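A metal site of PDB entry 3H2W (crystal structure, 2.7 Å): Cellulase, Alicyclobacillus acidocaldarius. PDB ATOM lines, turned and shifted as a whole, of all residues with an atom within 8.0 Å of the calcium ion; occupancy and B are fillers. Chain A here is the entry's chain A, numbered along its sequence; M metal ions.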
ATOM      1  N   VAL A 152     -25.632  10.712  16.306  1.00  0.00           N
ATOM      2  CA  VAL A 152     -24.570  10.209  17.170  1.00  0.00           C
ATOM      3  C   VAL A 152     -24.034   8.898  16.627  1.00  0.00           C
ATOM      4  O   VAL A 152     -22.861   8.856  16.228  1.00  0.00           O
ATOM      5  CB  VAL A 152     -25.016  10.071  18.648  1.00  0.00           C
ATOM      6  CG1 VAL A 152     -24.121   9.109  19.405  1.00  0.00           C
ATOM      7  CG2 VAL A 152     -25.038  11.449  19.323  1.00  0.00           C
ATOM      8  N   ALA A 243     -24.271  16.095  22.262  1.00  0.00           N
ATOM      9  CA  ALA A 243     -23.644  14.886  21.728  1.00  0.00           C
ATOM     10  C   ALA A 243     -23.712  14.832  20.189  1.00  0.00           C
ATOM     11  O   ALA A 243     -22.705  14.517  19.514  1.00  0.00           O
ATOM     12  CB  ALA A 243     -24.272  13.625  22.341  1.00  0.00           C
ATOM     13  N   THR A 247     -20.184  15.199  18.006  1.00  0.00           N
ATOM     14  CA  THR A 247     -19.857  14.050  17.146  1.00  0.00           C
ATOM     15  C   THR A 247     -19.937  14.417  15.652  1.00  0.00           C
ATOM     16  O   THR A 247     -19.161  13.921  14.836  1.00  0.00           O
ATOM     17  CB  THR A 247     -20.805  12.860  17.427  1.00  0.00           C
ATOM     18  OG1 THR A 247     -22.168  13.310  17.370  1.00  0.00           O
ATOM     19  CG2 THR A 247     -20.518  12.203  18.791  1.00  0.00           C
ATOM     20  N   GLY A 301     -28.666   8.050  24.299  1.00  0.00           N
ATOM     21  CA  GLY A 301     -28.321   9.002  25.350  1.00  0.00           C
ATOM     22  C   GLY A 301     -26.926   8.732  25.895  1.00  0.00           C
ATOM     23  O   GLY A 301     -26.301   7.716  25.566  1.00  0.00           O
ATOM     24  N   ASP A 302     -26.444   9.637  26.744  1.00  0.00           N
ATOM     25  CA  ASP A 302     -25.108   9.564  27.281  1.00  0.00           C
ATOM     26  C   ASP A 302     -24.983  10.657  28.373  1.00  0.00           C
ATOM     27  O   ASP A 302     -25.249  11.835  28.131  1.00  0.00           O
ATOM     28  CB  ASP A 302     -24.093   9.755  26.139  1.00  0.00           C
ATOM     29  CG  ASP A 302     -22.642   9.471  26.513  1.00  0.00           C
ATOM     30  OD1 ASP A 302     -22.315   9.037  27.640  1.00  0.00           O
ATOM     31  OD2 ASP A 302     -21.783   9.686  25.631  1.00  0.00           O
ATOM     32  N   ALA A 303     -24.657  10.244  29.603  1.00  0.00           N
ATOM     33  CA  ALA A 303     -24.407  11.172  30.703  1.00  0.00           C
ATOM     34  C   ALA A 303     -23.105  11.944  30.479  1.00  0.00           C
ATOM     35  O   ALA A 303     -23.026  13.130  30.775  1.00  0.00           O
ATOM     36  CB  ALA A 303     -24.363  10.407  32.038  1.00  0.00           C
ATOM     37  N   GLU A 304     -22.090  11.249  29.954  1.00  0.00           N
ATOM     38  CA  GLU A 304     -20.733  11.800  29.814  1.00  0.00           C
ATOM     39  C   GLU A 304     -20.499  12.365  28.415  1.00  0.00           C
ATOM     40  O   GLU A 304     -20.469  11.628  27.399  1.00  0.00           O
ATOM     41  CB  GLU A 304     -19.670  10.727  30.167  1.00  0.00           C
ATOM     42  CG  GLU A 304     -18.210  11.185  30.109  1.00  0.00           C
ATOM     43  CD  GLU A 304     -17.931  12.408  30.971  1.00  0.00           C
ATOM     44  OE1 GLU A 304     -18.112  12.345  32.193  1.00  0.00           O
ATOM     45  OE2 GLU A 304     -17.556  13.452  30.424  1.00  0.00           O
ATOM     46  N   LEU A 305     -20.312  13.686  28.379  1.00  0.00           N
ATOM     47  CA  LEU A 305     -20.160  14.408  27.138  1.00  0.00           C
ATOM     48  C   LEU A 305     -18.775  14.981  26.936  1.00  0.00           C
ATOM     49  O   LEU A 305     -18.563  15.726  25.978  1.00  0.00           O
ATOM     50  CB  LEU A 305     -21.194  15.541  27.094  1.00  0.00           C
ATOM     51  CG  LEU A 305     -22.625  15.012  26.983  1.00  0.00           C
ATOM     52  CD1 LEU A 305     -23.628  16.134  27.254  1.00  0.00           C
ATOM     53  CD2 LEU A 305     -22.846  14.324  25.596  1.00  0.00           C
ATOM     54  N   ARG A 306     -17.826  14.642  27.799  1.00  0.00           N
ATOM     55  CA  ARG A 306     -16.493  15.218  27.674  1.00  0.00           C
ATOM     56  C   ARG A 306     -15.663  14.528  26.617  1.00  0.00           C
ATOM     57  O   ARG A 306     -14.815  15.175  25.977  1.00  0.00           O
ATOM     58  CB  ARG A 306     -15.779  15.218  29.004  1.00  0.00           C
ATOM     59  CG  ARG A 306     -16.419  16.180  29.966  1.00  0.00           C
ATOM     60  CD  ARG A 306     -15.776  16.155  31.276  1.00  0.00           C
ATOM     61  NE  ARG A 306     -16.143  14.958  32.009  1.00  0.00           N
ATOM     62  CZ  ARG A 306     -15.504  14.525  33.091  1.00  0.00           C
ATOM     63  NH1 ARG A 306     -14.476  15.222  33.594  1.00  0.00           N
ATOM     64  NH2 ARG A 306     -15.909  13.422  33.713  1.00  0.00           N
ATOM     65  N   ASP A 307     -15.889  13.231  26.454  1.00  0.00           N
ATOM     66  CA  ASP A 307     -15.174  12.448  25.447  1.00  0.00           C
ATOM     67  C   ASP A 307     -15.538  12.918  24.046  1.00  0.00           C
ATOM     68  O   ASP A 307     -14.723  12.850  23.115  1.00  0.00           O
ATOM     69  CB  ASP A 307     -15.453  10.936  25.585  1.00  0.00           C
ATOM     70  CG  ASP A 307     -16.927  10.618  25.710  1.00  0.00           C
ATOM     71  OD1 ASP A 307     -17.529  10.938  26.761  1.00  0.00           O
ATOM     72  OD2 ASP A 307     -17.487  10.034  24.754  1.00  0.00           O
ATOM     73  N   GLU A 308     -16.785  13.377  23.914  1.00  0.00           N
ATOM     74  CA  GLU A 308     -17.280  13.927  22.648  1.00  0.00           C
ATOM     75  C   GLU A 308     -16.556  15.242  22.359  1.00  0.00           C
ATOM     76  O   GLU A 308     -16.109  15.448  21.239  1.00  0.00           O
ATOM     77  CB  GLU A 308     -18.801  14.130  22.675  1.00  0.00           C
ATOM     78  CG  GLU A 308     -19.643  12.826  22.560  1.00  0.00           C
ATOM     79  CD  GLU A 308     -19.663  11.992  23.845  1.00  0.00           C
ATOM     80  OE1 GLU A 308     -19.244  12.483  24.910  1.00  0.00           O
ATOM     81  OE2 GLU A 308     -20.048  10.808  23.812  1.00  0.00           O
ATOM     82  N   LEU A 309     -16.419  16.113  23.380  1.00  0.00           N
ATOM     83  CA  LEU A 309     -15.622  17.346  23.253  1.00  0.00           C
ATOM     84  C   LEU A 309     -14.169  17.065  22.897  1.00  0.00           C
ATOM     85  O   LEU A 309     -13.593  17.731  22.051  1.00  0.00           O
ATOM     86  CB  LEU A 309     -15.681  18.195  24.529  1.00  0.00           C
ATOM     87  CG  LEU A 309     -15.009  19.574  24.405  1.00  0.00           C
ATOM     88  CD1 LEU A 309     -15.557  20.307  23.192  1.00  0.00           C
ATOM     89  CD2 LEU A 309     -15.154  20.441  25.662  1.00  0.00           C
ATOM     90  N   LEU A 337     -11.216   9.361  31.177  1.00  0.00           N
ATOM     91  CA  LEU A 337     -12.295   8.874  30.298  1.00  0.00           C
ATOM     92  C   LEU A 337     -11.915   7.499  29.751  1.00  0.00           C
ATOM     93  O   LEU A 337     -10.724   7.210  29.626  1.00  0.00           O
ATOM     94  CB  LEU A 337     -12.520   9.850  29.153  1.00  0.00           C
ATOM     95  CG  LEU A 337     -13.174  11.162  29.573  1.00  0.00           C
ATOM     96  CD1 LEU A 337     -13.141  12.204  28.456  1.00  0.00           C
ATOM     97  CD2 LEU A 337     -14.594  10.922  30.010  1.00  0.00           C
ATOM     98  N   PRO A 338     -12.895   6.634  29.434  1.00  0.00           N
ATOM     99  CA  PRO A 338     -12.478   5.378  28.806  1.00  0.00           C
ATOM    100  C   PRO A 338     -12.153   5.653  27.352  1.00  0.00           C
ATOM    101  O   PRO A 338     -12.845   6.451  26.695  1.00  0.00           O
ATOM    102  CB  PRO A 338     -13.689   4.455  28.944  1.00  0.00           C
ATOM    103  CG  PRO A 338     -14.821   5.304  29.459  1.00  0.00           C
ATOM    104  CD  PRO A 338     -14.364   6.725  29.600  1.00  0.00           C
ATOM    105  N   TRP A 343     -20.424   3.596  20.557  1.00  0.00           N
ATOM    106  CA  TRP A 343     -20.960   4.867  20.040  1.00  0.00           C
ATOM    107  C   TRP A 343     -21.015   6.022  21.053  1.00  0.00           C
ATOM    108  O   TRP A 343     -20.988   7.201  20.657  1.00  0.00           O
ATOM    109  CB  TRP A 343     -22.343   4.651  19.403  1.00  0.00           C
ATOM    110  CG  TRP A 343     -23.392   4.107  20.331  1.00  0.00           C
ATOM    111  CD1 TRP A 343     -23.763   2.805  20.448  1.00  0.00           C
ATOM    112  CD2 TRP A 343     -24.215   4.841  21.237  1.00  0.00           C
ATOM    113  NE1 TRP A 343     -24.751   2.680  21.380  1.00  0.00           N
ATOM    114  CE2 TRP A 343     -25.059   3.911  21.886  1.00  0.00           C
ATOM    115  CE3 TRP A 343     -24.330   6.205  21.574  1.00  0.00           C
ATOM    116  CZ2 TRP A 343     -25.987   4.290  22.857  1.00  0.00           C
ATOM    117  CZ3 TRP A 343     -25.255   6.584  22.555  1.00  0.00           C
ATOM    118  CH2 TRP A 343     -26.082   5.618  23.171  1.00  0.00           C
ATOM    119  N   ALA A 344     -21.080   5.680  22.346  1.00  0.00           N
ATOM    120  CA  ALA A 344     -21.171   6.678  23.464  1.00  0.00           C
ATOM    121  C   ALA A 344     -19.811   7.148  23.996  1.00  0.00           C
ATOM    122  O   ALA A 344     -19.626   8.337  24.335  1.00  0.00           O
ATOM    123  CB  ALA A 344     -22.006   6.133  24.603  1.00  0.00           C
ATOM    124  N   ASP A 345     -18.891   6.206  24.099  1.00  0.00           N
ATOM    125  CA  ASP A 345     -17.583   6.483  24.659  1.00  0.00           C
ATOM    126  C   ASP A 345     -16.674   6.506  23.444  1.00  0.00           C
ATOM    127  O   ASP A 345     -16.343   5.456  22.856  1.00  0.00           O
ATOM    128  CB  ASP A 345     -17.164   5.398  25.652  1.00  0.00           C
ATOM    129  CG  ASP A 345     -18.198   5.173  26.740  1.00  0.00           C
ATOM    130  OD1 ASP A 345     -18.982   4.225  26.613  1.00  0.00           O
ATOM    131  OD2 ASP A 345     -18.222   5.918  27.733  1.00  0.00           O
ATOM    132  N   VAL A 346     -16.309   7.713  23.086  1.00  0.00           N
ATOM    133  CA  VAL A 346     -15.705   8.005  21.802  1.00  0.00           C
ATOM    134  C   VAL A 346     -14.279   8.576  21.911  1.00  0.00           C
ATOM    135  O   VAL A 346     -13.675   8.909  20.915  1.00  0.00           O
ATOM    136  CB  VAL A 346     -16.600   9.009  21.062  1.00  0.00           C
ATOM    137  CG1 VAL A 346     -17.901   8.360  20.725  1.00  0.00           C
ATOM    138  CG2 VAL A 346     -16.825  10.275  21.895  1.00  0.00           C
ATOM    139  N   ALA A 347     -13.736   8.693  23.124  1.00  0.00           N
ATOM    140  CA  ALA A 347     -12.401   9.276  23.352  1.00  0.00           C
ATOM    141  C   ALA A 347     -11.315   8.705  22.445  1.00  0.00           C
ATOM    142  O   ALA A 347     -10.472   9.437  21.935  1.00  0.00           O
ATOM    143  CB  ALA A 347     -12.000   9.092  24.815  1.00  0.00           C
HETATM  144 CA    CA M   1     -19.704  10.122  25.828  1.00  0.00          CA
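OE2 of Glu 304 lies within salt-bridge range of NE of Arg 306 (2.6 Å). OD2 of Asp 307 sits close to N of Val 346, at 3.1 Å.
The nearest printed residue that does not touch the calcium ion is Asp 345 (4.4 Å).
The calcium ion is bound by OD2 of Asp 302, at 2.1 Å. OE2 of Glu 308 binds the calcium ion, at 2.2 Å. O of Glu 304 binds the calcium ion (2.3 Å). The calcium ion is bound by O of Ala 344. The calcium ion is bound by OD2 of Asp 307. OD1 of Asp 307 binds the calcium ion, at 2.5 Å. The calcium ion is bound by OE1 of Glu 308, at 2.6 Å. The calcium ion has seven donor atoms within binding distance.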
